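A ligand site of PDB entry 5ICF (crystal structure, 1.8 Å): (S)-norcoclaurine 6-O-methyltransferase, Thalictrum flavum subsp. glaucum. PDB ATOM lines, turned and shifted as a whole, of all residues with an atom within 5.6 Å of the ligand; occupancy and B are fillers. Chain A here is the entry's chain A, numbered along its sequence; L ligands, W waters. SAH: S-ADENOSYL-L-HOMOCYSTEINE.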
ATOM      1  N   TRP A 151      17.901 -20.149  32.144  1.00  0.00           N
ATOM      2  CA  TRP A 151      17.923 -20.386  30.685  1.00  0.00           C
ATOM      3  C   TRP A 151      17.456 -19.147  29.874  1.00  0.00           C
ATOM      4  O   TRP A 151      18.068 -18.808  28.879  1.00  0.00           O
ATOM      5  CB  TRP A 151      17.046 -21.645  30.289  1.00  0.00           C
ATOM      6  CG  TRP A 151      17.445 -22.830  31.233  1.00  0.00           C
ATOM      7  CD1 TRP A 151      16.594 -23.489  32.061  1.00  0.00           C
ATOM      8  CD2 TRP A 151      18.780 -23.310  31.539  1.00  0.00           C
ATOM      9  NE1 TRP A 151      17.286 -24.451  32.787  1.00  0.00           N
ATOM     10  CE2 TRP A 151      18.627 -24.352  32.504  1.00  0.00           C
ATOM     11  CE3 TRP A 151      20.053 -22.987  31.092  1.00  0.00           C
ATOM     12  CZ2 TRP A 151      19.724 -25.078  33.015  1.00  0.00           C
ATOM     13  CZ3 TRP A 151      21.163 -23.665  31.645  1.00  0.00           C
ATOM     14  CH2 TRP A 151      20.981 -24.717  32.581  1.00  0.00           C
ATOM     15  N   PHE A 164      28.836 -18.906  30.463  1.00  0.00           N
ATOM     16  CA  PHE A 164      28.253 -20.152  31.013  1.00  0.00           C
ATOM     17  C   PHE A 164      28.619 -21.359  30.108  1.00  0.00           C
ATOM     18  O   PHE A 164      29.114 -22.416  30.582  1.00  0.00           O
ATOM     19  CB  PHE A 164      26.744 -20.047  31.078  1.00  0.00           C
ATOM     20  CG  PHE A 164      26.078 -21.361  31.518  1.00  0.00           C
ATOM     21  CD1 PHE A 164      25.898 -21.650  32.868  1.00  0.00           C
ATOM     22  CD2 PHE A 164      25.770 -22.326  30.605  1.00  0.00           C
ATOM     23  CE1 PHE A 164      25.289 -22.841  33.283  1.00  0.00           C
ATOM     24  CE2 PHE A 164      25.226 -23.554  31.016  1.00  0.00           C
ATOM     25  CZ  PHE A 164      24.968 -23.788  32.324  1.00  0.00           C
ATOM     26  N   ASN A 165      28.423 -21.182  28.797  1.00  0.00           N
ATOM     27  CA  ASN A 165      28.704 -22.292  27.862  1.00  0.00           C
ATOM     28  C   ASN A 165      30.161 -22.709  27.885  1.00  0.00           C
ATOM     29  O   ASN A 165      30.475 -23.870  27.753  1.00  0.00           O
ATOM     30  CB  ASN A 165      28.323 -21.903  26.443  1.00  0.00           C
ATOM     31  CG  ASN A 165      26.831 -21.649  26.295  1.00  0.00           C
ATOM     32  OD1 ASN A 165      26.008 -22.201  27.060  1.00  0.00           O
ATOM     33  ND2 ASN A 165      26.467 -20.863  25.246  1.00  0.00           N
ATOM     34  N   MET A 168      30.893 -24.812  31.005  1.00  0.00           N
ATOM     35  CA  MET A 168      30.414 -26.198  30.789  1.00  0.00           C
ATOM     36  C   MET A 168      31.306 -26.899  29.754  1.00  0.00           C
ATOM     37  O   MET A 168      31.598 -28.102  29.913  1.00  0.00           O
ATOM     38  CB  MET A 168      28.944 -26.225  30.330  1.00  0.00           C
ATOM     39  CG  MET A 168      27.970 -25.736  31.455  1.00  0.00           C
ATOM     40  SD  MET A 168      28.250 -26.480  33.070  1.00  0.00           S
ATOM     41  CE  MET A 168      27.950 -28.225  32.781  1.00  0.00           C
ATOM     42  N   ALA A 169      31.729 -26.178  28.692  1.00  0.00           N
ATOM     43  CA  ALA A 169      32.660 -26.799  27.724  1.00  0.00           C
ATOM     44  C   ALA A 169      33.904 -27.284  28.498  1.00  0.00           C
ATOM     45  O   ALA A 169      34.417 -28.329  28.224  1.00  0.00           O
ATOM     46  CB  ALA A 169      33.064 -25.795  26.637  1.00  0.00           C
ATOM     47  N   ASP A 171      34.176 -28.046  31.775  1.00  0.00           N
ATOM     48  CA  ASP A 171      33.857 -29.208  32.617  1.00  0.00           C
ATOM     49  C   ASP A 171      33.817 -30.478  31.735  1.00  0.00           C
ATOM     50  O   ASP A 171      34.277 -31.552  32.150  1.00  0.00           O
ATOM     51  CB  ASP A 171      32.494 -29.021  33.221  1.00  0.00           C
ATOM     52  CG  ASP A 171      32.094 -30.213  34.163  1.00  0.00           C
ATOM     53  OD1 ASP A 171      32.875 -30.480  35.097  1.00  0.00           O
ATOM     54  OD2 ASP A 171      31.150 -30.921  33.843  1.00  0.00           O
ATOM     55  N   THR A 172      33.285 -30.368  30.517  1.00  0.00           N
ATOM     56  CA  THR A 172      33.257 -31.504  29.568  1.00  0.00           C
ATOM     57  C   THR A 172      34.623 -31.946  29.135  1.00  0.00           C
ATOM     58  O   THR A 172      34.916 -33.170  29.086  1.00  0.00           O
ATOM     59  CB  THR A 172      32.357 -31.148  28.342  1.00  0.00           C
ATOM     60  OG1 THR A 172      31.056 -30.841  28.864  1.00  0.00           O
ATOM     61  CG2 THR A 172      32.254 -32.379  27.370  1.00  0.00           C
ATOM     62  N   ASP A 195      23.368 -35.836  21.688  1.00  0.00           N
ATOM     63  CA  ASP A 195      23.682 -35.259  23.034  1.00  0.00           C
ATOM     64  C   ASP A 195      22.660 -34.205  23.348  1.00  0.00           C
ATOM     65  O   ASP A 195      22.676 -33.071  22.795  1.00  0.00           O
ATOM     66  CB  ASP A 195      25.084 -34.692  22.975  1.00  0.00           C
ATOM     67  CG  ASP A 195      25.606 -34.289  24.348  1.00  0.00           C
ATOM     68  OD1 ASP A 195      24.953 -34.629  25.322  1.00  0.00           O
ATOM     69  OD2 ASP A 195      26.658 -33.645  24.391  1.00  0.00           O
ATOM     70  N   VAL A 196      21.688 -34.574  24.172  1.00  0.00           N
ATOM     71  CA  VAL A 196      20.529 -33.708  24.448  1.00  0.00           C
ATOM     72  C   VAL A 196      20.966 -32.687  25.488  1.00  0.00           C
ATOM     73  O   VAL A 196      21.496 -33.078  26.570  1.00  0.00           O
ATOM     74  CB  VAL A 196      19.353 -34.598  24.990  1.00  0.00           C
ATOM     75  CG1 VAL A 196      18.281 -33.773  25.611  1.00  0.00           C
ATOM     76  CG2 VAL A 196      18.769 -35.421  23.792  1.00  0.00           C
ATOM     77  N   GLY A 197      20.700 -31.386  25.204  1.00  0.00           N
ATOM     78  CA  GLY A 197      21.280 -30.323  26.066  1.00  0.00           C
ATOM     79  C   GLY A 197      22.820 -30.328  25.896  1.00  0.00           C
ATOM     80  O   GLY A 197      23.514 -30.126  26.861  1.00  0.00           O
ATOM     81  N   GLY A 198      23.304 -30.614  24.652  1.00  0.00           N
ATOM     82  CA  GLY A 198      24.761 -30.986  24.465  1.00  0.00           C
ATOM     83  C   GLY A 198      25.676 -29.737  24.531  1.00  0.00           C
ATOM     84  O   GLY A 198      26.905 -29.824  24.253  1.00  0.00           O
ATOM     85  N   GLY A 199      25.072 -28.534  24.818  1.00  0.00           N
ATOM     86  CA  GLY A 199      25.950 -27.321  24.963  1.00  0.00           C
ATOM     87  C   GLY A 199      26.460 -26.934  23.630  1.00  0.00           C
ATOM     88  O   GLY A 199      25.767 -27.089  22.603  1.00  0.00           O
ATOM     89  N   TYR A 219      22.258 -31.149  20.443  1.00  0.00           N
ATOM     90  CA  TYR A 219      20.904 -30.573  20.522  1.00  0.00           C
ATOM     91  C   TYR A 219      20.837 -29.720  21.763  1.00  0.00           C
ATOM     92  O   TYR A 219      21.175 -30.192  22.849  1.00  0.00           O
ATOM     93  CB  TYR A 219      19.928 -31.741  20.653  1.00  0.00           C
ATOM     94  CG  TYR A 219      18.451 -31.394  20.844  1.00  0.00           C
ATOM     95  CD1 TYR A 219      17.825 -30.421  20.052  1.00  0.00           C
ATOM     96  CD2 TYR A 219      17.661 -32.128  21.702  1.00  0.00           C
ATOM     97  CE1 TYR A 219      16.434 -30.130  20.203  1.00  0.00           C
ATOM     98  CE2 TYR A 219      16.302 -31.859  21.843  1.00  0.00           C
ATOM     99  CZ  TYR A 219      15.700 -30.860  21.092  1.00  0.00           C
ATOM    100  OH  TYR A 219      14.356 -30.568  21.208  1.00  0.00           O
ATOM    101  N   ASP A 220      20.419 -28.466  21.589  1.00  0.00           N
ATOM    102  CA  ASP A 220      20.296 -27.545  22.734  1.00  0.00           C
ATOM    103  C   ASP A 220      19.307 -26.416  22.345  1.00  0.00           C
ATOM    104  O   ASP A 220      18.708 -26.430  21.257  1.00  0.00           O
ATOM    105  CB  ASP A 220      21.667 -26.920  23.105  1.00  0.00           C
ATOM    106  CG  ASP A 220      21.749 -26.635  24.637  1.00  0.00           C
ATOM    107  OD1 ASP A 220      21.053 -25.710  25.053  1.00  0.00           O
ATOM    108  OD2 ASP A 220      22.578 -27.262  25.351  1.00  0.00           O
ATOM    109  N   LEU A 221      19.202 -25.429  23.221  1.00  0.00           N
ATOM    110  CA  LEU A 221      18.287 -24.284  22.937  1.00  0.00           C
ATOM    111  C   LEU A 221      18.922 -23.432  21.909  1.00  0.00           C
ATOM    112  O   LEU A 221      20.132 -23.419  21.736  1.00  0.00           O
ATOM    113  CB  LEU A 221      18.091 -23.454  24.252  1.00  0.00           C
ATOM    114  CG  LEU A 221      17.400 -24.231  25.411  1.00  0.00           C
ATOM    115  CD1 LEU A 221      17.564 -23.505  26.755  1.00  0.00           C
ATOM    116  CD2 LEU A 221      15.898 -24.399  25.056  1.00  0.00           C
ATOM    117  N   HIS A 223      19.646 -20.225  21.585  1.00  0.00           N
ATOM    118  CA  HIS A 223      20.764 -19.310  21.978  1.00  0.00           C
ATOM    119  C   HIS A 223      22.111 -20.017  22.276  1.00  0.00           C
ATOM    120  O   HIS A 223      23.178 -19.408  22.166  1.00  0.00           O
ATOM    121  CB  HIS A 223      20.351 -18.400  23.160  1.00  0.00           C
ATOM    122  CG  HIS A 223      20.071 -19.131  24.456  1.00  0.00           C
ATOM    123  ND1 HIS A 223      18.809 -19.588  24.795  1.00  0.00           N
ATOM    124  CD2 HIS A 223      20.912 -19.589  25.407  1.00  0.00           C
ATOM    125  CE1 HIS A 223      18.878 -20.243  25.947  1.00  0.00           C
ATOM    126  NE2 HIS A 223      20.129 -20.204  26.370  1.00  0.00           N
ATOM    127  N   VAL A 224      22.069 -21.333  22.565  1.00  0.00           N
ATOM    128  CA  VAL A 224      23.287 -22.070  22.780  1.00  0.00           C
ATOM    129  C   VAL A 224      23.828 -22.606  21.449  1.00  0.00           C
ATOM    130  O   VAL A 224      25.056 -22.552  21.182  1.00  0.00           O
ATOM    131  CB  VAL A 224      23.017 -23.255  23.807  1.00  0.00           C
ATOM    132  CG1 VAL A 224      24.283 -24.117  23.932  1.00  0.00           C
ATOM    133  CG2 VAL A 224      22.587 -22.705  25.140  1.00  0.00           C
ATOM    134  N   GLY A 239      16.098 -26.616  19.805  1.00  0.00           N
ATOM    135  CA  GLY A 239      14.725 -26.920  20.197  1.00  0.00           C
ATOM    136  C   GLY A 239      14.578 -27.018  21.702  1.00  0.00           C
ATOM    137  O   GLY A 239      15.391 -26.517  22.469  1.00  0.00           O
ATOM    138  N   ASP A 240      13.499 -27.664  22.146  1.00  0.00           N
ATOM    139  CA  ASP A 240      13.178 -27.740  23.550  1.00  0.00           C
ATOM    140  C   ASP A 240      13.031 -29.257  23.807  1.00  0.00           C
ATOM    141  O   ASP A 240      12.072 -29.900  23.334  1.00  0.00           O
ATOM    142  CB  ASP A 240      11.844 -26.995  23.784  1.00  0.00           C
ATOM    143  CG  ASP A 240      11.336 -27.105  25.176  1.00  0.00           C
ATOM    144  OD1 ASP A 240      11.985 -27.723  26.039  1.00  0.00           O
ATOM    145  OD2 ASP A 240      10.214 -26.587  25.433  1.00  0.00           O
ATOM    146  N   MET A 241      13.917 -29.781  24.680  1.00  0.00           N
ATOM    147  CA  MET A 241      13.919 -31.230  24.964  1.00  0.00           C
ATOM    148  C   MET A 241      12.634 -31.691  25.687  1.00  0.00           C
ATOM    149  O   MET A 241      12.305 -32.855  25.675  1.00  0.00           O
ATOM    150  CB  MET A 241      15.140 -31.608  25.838  1.00  0.00           C
ATOM    151  CG  MET A 241      15.039 -31.013  27.240  1.00  0.00           C
ATOM    152  SD  MET A 241      16.667 -31.187  28.102  1.00  0.00           S
ATOM    153  CE  MET A 241      16.305 -30.184  29.552  1.00  0.00           C
ATOM    154  N   PHE A 242      11.888 -30.744  26.277  1.00  0.00           N
ATOM    155  CA  PHE A 242      10.618 -31.089  26.875  1.00  0.00           C
ATOM    156  C   PHE A 242       9.512 -31.371  25.860  1.00  0.00           C
ATOM    157  O   PHE A 242       8.484 -31.994  26.209  1.00  0.00           O
ATOM    158  CB  PHE A 242      10.133 -30.001  27.839  1.00  0.00           C
ATOM    159  CG  PHE A 242      10.889 -30.049  29.121  1.00  0.00           C
ATOM    160  CD1 PHE A 242      10.580 -31.006  30.075  1.00  0.00           C
ATOM    161  CD2 PHE A 242      11.955 -29.184  29.348  1.00  0.00           C
ATOM    162  CE1 PHE A 242      11.296 -31.100  31.304  1.00  0.00           C
ATOM    163  CE2 PHE A 242      12.695 -29.270  30.560  1.00  0.00           C
ATOM    164  CZ  PHE A 242      12.323 -30.210  31.528  1.00  0.00           C
ATOM    165  N   MET A 253      22.948 -37.524  28.025  1.00  0.00           N
ATOM    166  CA  MET A 253      22.602 -36.263  28.759  1.00  0.00           C
ATOM    167  C   MET A 253      23.660 -36.073  29.839  1.00  0.00           C
ATOM    168  O   MET A 253      23.702 -36.835  30.811  1.00  0.00           O
ATOM    169  CB  MET A 253      21.199 -36.350  29.407  1.00  0.00           C
ATOM    170  CG  MET A 253      20.039 -36.296  28.408  1.00  0.00           C
ATOM    171  SD  MET A 253      18.453 -36.306  29.235  1.00  0.00           S
ATOM    172  CE  MET A 253      18.424 -38.039  29.823  1.00  0.00           C
ATOM    173  N   LYS A 254      24.525 -35.063  29.616  1.00  0.00           N
ATOM    174  CA  LYS A 254      25.493 -34.728  30.660  1.00  0.00           C
ATOM    175  C   LYS A 254      25.141 -33.419  31.343  1.00  0.00           C
ATOM    176  O   LYS A 254      24.880 -32.428  30.648  1.00  0.00           O
ATOM    177  CB  LYS A 254      26.923 -34.612  30.030  1.00  0.00           C
ATOM    178  CG  LYS A 254      27.906 -34.098  31.085  1.00  0.00           C
ATOM    179  CD  LYS A 254      29.352 -33.958  30.475  1.00  0.00           C
ATOM    180  CE  LYS A 254      30.251 -33.223  31.451  1.00  0.00           C
ATOM    181  NZ  LYS A 254      29.971 -31.736  31.567  1.00  0.00           N
ATOM    182  N   CYS A 255      25.053 -33.478  32.697  1.00  0.00           N
ATOM    183  CA  CYS A 255      24.713 -32.296  33.500  1.00  0.00           C
ATOM    184  C   CYS A 255      23.401 -31.689  33.004  1.00  0.00           C
ATOM    185  O   CYS A 255      23.247 -30.461  32.978  1.00  0.00           O
ATOM    186  CB  CYS A 255      25.893 -31.234  33.425  1.00  0.00           C
ATOM    187  SG  CYS A 255      27.397 -31.932  34.211  1.00  0.00           S
ATOM    188  N   ILE A 256      22.415 -32.567  32.749  1.00  0.00           N
ATOM    189  CA  ILE A 256      21.102 -32.155  32.366  1.00  0.00           C
ATOM    190  C   ILE A 256      20.156 -32.450  33.529  1.00  0.00           C
ATOM    191  O   ILE A 256      19.459 -31.541  33.989  1.00  0.00           O
ATOM    192  CB  ILE A 256      20.613 -32.876  31.084  1.00  0.00           C
ATOM    193  CG1 ILE A 256      21.562 -32.649  29.891  1.00  0.00           C
ATOM    194  CG2 ILE A 256      19.156 -32.458  30.701  1.00  0.00           C
ATOM    195  CD1 ILE A 256      21.866 -31.160  29.600  1.00  0.00           C
ATOM    196  N   ASP A 259      19.600 -30.532  36.684  1.00  0.00           N
ATOM    197  CA  ASP A 259      18.969 -29.184  36.588  1.00  0.00           C
ATOM    198  C   ASP A 259      17.504 -29.212  36.891  1.00  0.00           C
ATOM    199  O   ASP A 259      16.848 -28.129  37.007  1.00  0.00           O
ATOM    200  CB  ASP A 259      19.114 -28.619  35.148  1.00  0.00           C
ATOM    201  CG  ASP A 259      20.556 -28.288  34.762  1.00  0.00           C
ATOM    202  OD1 ASP A 259      21.371 -27.991  35.670  1.00  0.00           O
ATOM    203  OD2 ASP A 259      20.833 -28.233  33.545  1.00  0.00           O
ATOM    204  N   TRP A 260      16.897 -30.383  37.027  1.00  0.00           N
ATOM    205  CA  TRP A 260      15.417 -30.479  37.035  1.00  0.00           C
ATOM    206  C   TRP A 260      14.882 -31.266  38.219  1.00  0.00           C
ATOM    207  O   TRP A 260      15.599 -32.081  38.791  1.00  0.00           O
ATOM    208  CB  TRP A 260      14.940 -31.128  35.723  1.00  0.00           C
ATOM    209  CG  TRP A 260      15.427 -30.361  34.540  1.00  0.00           C
ATOM    210  CD1 TRP A 260      16.494 -30.682  33.789  1.00  0.00           C
ATOM    211  CD2 TRP A 260      14.926 -29.115  34.026  1.00  0.00           C
ATOM    212  NE1 TRP A 260      16.705 -29.756  32.809  1.00  0.00           N
ATOM    213  CE2 TRP A 260      15.768 -28.760  32.935  1.00  0.00           C
ATOM    214  CE3 TRP A 260      13.899 -28.257  34.407  1.00  0.00           C
ATOM    215  CZ2 TRP A 260      15.602 -27.591  32.169  1.00  0.00           C
ATOM    216  CZ3 TRP A 260      13.686 -27.082  33.616  1.00  0.00           C
ATOM    217  CH2 TRP A 260      14.571 -26.764  32.523  1.00  0.00           C
HETATM  218  N   SAH L   1      25.683 -31.122  28.360  1.00  0.00           N
HETATM  219  CA  SAH L   1      26.535 -29.878  28.476  1.00  0.00           C
HETATM  220  CB  SAH L   1      25.699 -28.719  29.026  1.00  0.00           C
HETATM  221  CG  SAH L   1      25.159 -28.931  30.444  1.00  0.00           C
HETATM  222  SD  SAH L   1      24.413 -27.440  31.088  1.00  0.00           S
HETATM  223  C   SAH L   1      27.746 -30.136  29.407  1.00  0.00           C
HETATM  224  O   SAH L   1      28.821 -29.462  29.282  1.00  0.00           O
HETATM  225  OXT SAH L   1      27.689 -30.959  30.302  1.00  0.00           O
HETATM  226  C5' SAH L   1      22.686 -27.696  30.766  1.00  0.00           C
HETATM  227  C4' SAH L   1      22.355 -27.541  29.228  1.00  0.00           C
HETATM  228  O4' SAH L   1      20.908 -27.801  29.144  1.00  0.00           O
HETATM  229  C3' SAH L   1      22.536 -26.068  28.752  1.00  0.00           C
HETATM  230  O3' SAH L   1      23.386 -26.051  27.603  1.00  0.00           O
HETATM  231  C2' SAH L   1      21.124 -25.548  28.494  1.00  0.00           C
HETATM  232  O2' SAH L   1      21.058 -24.590  27.444  1.00  0.00           O
HETATM  233  C1' SAH L   1      20.419 -26.873  28.121  1.00  0.00           C
HETATM  234  N9  SAH L   1      18.967 -26.750  28.244  1.00  0.00           N
HETATM  235  C8  SAH L   1      18.251 -26.173  29.220  1.00  0.00           C
HETATM  236  N7  SAH L   1      16.916 -26.320  28.977  1.00  0.00           N
HETATM  237  C5  SAH L   1      16.805 -26.970  27.773  1.00  0.00           C
HETATM  238  C6  SAH L   1      15.655 -27.409  26.943  1.00  0.00           C
HETATM  239  N6  SAH L   1      14.383 -27.155  27.356  1.00  0.00           N
HETATM  240  N1  SAH L   1      15.954 -28.163  25.847  1.00  0.00           N
HETATM  241  C2  SAH L   1      17.224 -28.348  25.464  1.00  0.00           C
HETATM  242  N3  SAH L   1      18.316 -27.947  26.201  1.00  0.00           N
HETATM  243  C4  SAH L   1      18.119 -27.302  27.358  1.00  0.00           C
HETATM  244  O   HOH W   1      25.937 -24.982  27.620  1.00  0.00           O
HETATM  245  O   HOH W   2      14.530 -24.959  29.410  1.00  0.00           O
HETATM  246  O   HOH W   3      23.899 -27.841  34.348  1.00  0.00           O
HETATM  247  O   HOH W   4      24.175 -33.265  27.416  1.00  0.00           O
HETATM  248  O   HOH W   5      21.373 -21.825  28.275  1.00  0.00           O
HETATM  249  O   HOH W   6      19.183 -28.780  31.310  1.00  0.00           O
HETATM  250  O   HOH W   7      27.428 -32.655  26.852  1.00  0.00           O
HETATM  251  O   HOH W   8      29.354 -28.186  26.949  1.00  0.00           O
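Water W1 lies within hydrogen-bond range of O3' of the ligand (2.8 Å) and OD1 of Asn 165 (2.8 Å).
Water W7 lies within hydrogen-bond range of OD2 of Asp 195 (2.8 Å) and N of the ligand (2.8 Å).
Water W5 lies within hydrogen-bond range of NE2 of His 223 (2.8 Å) and O2' of the ligand (2.9 Å).
Water W6 lies within hydrogen-bond range of OD2 of Asp 259 (2.8 Å), O4' of the ligand (2.9 Å) and NE1 of Trp 260 (3.1 Å).
OD2 of Asp 220 is in hydrogen-bond range of N of Gly 199 (2.8 Å).
OD2 of Asp 220 lies within hydrogen-bond range of N of Gly 198, at 3.5 Å.
OG1 of Thr 172 sits at hydrogen-bond distance from NZ of Lys 254 (3.0 Å).
O of Met 168 sits at hydrogen-bond distance from OG1 of Thr 172, 3.0 Å away.
The side-chain amino group of Lys 254 sits at hydrogen-bond distance from the side-chain sulfur of Cys 255, 3.7 Å away.
The backbone NH of Phe 242 sits at hydrogen-bond distance from the side-chain carboxylate of Asp 240 (3.0 Å).
The backbone NH of Gly 197 lies within hydrogen-bond range of the backbone carbonyl oxygen of Tyr 219 (2.7 Å).
The indole nitrogen of Trp 260 sits close to the backbone carbonyl oxygen of Ile 256, 3.5 Å away.
The side-chain carboxylate (OD1) of Asp 220 is in hydrogen-bond range of an oxygen (O2') of the ligand (2.6 Å).
The side-chain hydroxyl of Thr 172 lies within hydrogen-bond range of an oxygen (O) of the ligand.
O of Lys 254 lies within hydrogen-bond range of N of the ligand.
The side-chain amino group (NZ) of Lys 254 is in salt-bridge range of an oxygen (OXT) of the ligand.
OD1 of Asp 240 sits at hydrogen-bond distance from N6 of the ligand (2.8 Å).
The backbone carbonyl oxygen of Gly 197 sits at hydrogen-bond distance from a nitrogen (N) of the ligand (2.8 Å).
The backbone NH (N) of Met 241 sits at hydrogen-bond distance from a nitrogen (N1) of the ligand, at 2.9 Å.
O of Met 168 sits close to O of the ligand (3.2 Å).
The backbone carbonyl oxygen (O) of Cys 255 sits close to a sulfur (SD) of the ligand (3.7 Å).
Trp 151 touches the ligand (CZ3 to C2', 3.7 Å).
Phe 164 touches the ligand.
Gly 199 touches the ligand.
Leu 221 touches the ligand.
CG2 of Val 224 touches O2' of the ligand (3.3 Å).
O of Gly 239 touches N1 of the ligand (3.8 Å).
CD2 of Phe 242 touches N6 of the ligand, 3.7 Å away.
Ile 256 touches the ligand.
Asp 259 touches the ligand.
Trp 260 touches the ligand (CZ2 to N7, 3.7 Å).
Hydrophobic or aromatic side chains that line the ligand: Trp 151, Phe 164, Met 168, Leu 221, Val 224, Met 241, Phe 242, Ile 256 and Trp 260.
18 residues have an atom within 4 Å of the ligand: Trp 151, Phe 164, Met 168, Thr 172, Gly 197, Gly 199, Asp 220, Leu 221, Val 224, Gly 239, Asp 240, Met 241, Phe 242, Lys 254, Cys 255, Ile 256, Asp 259 and Trp 260.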
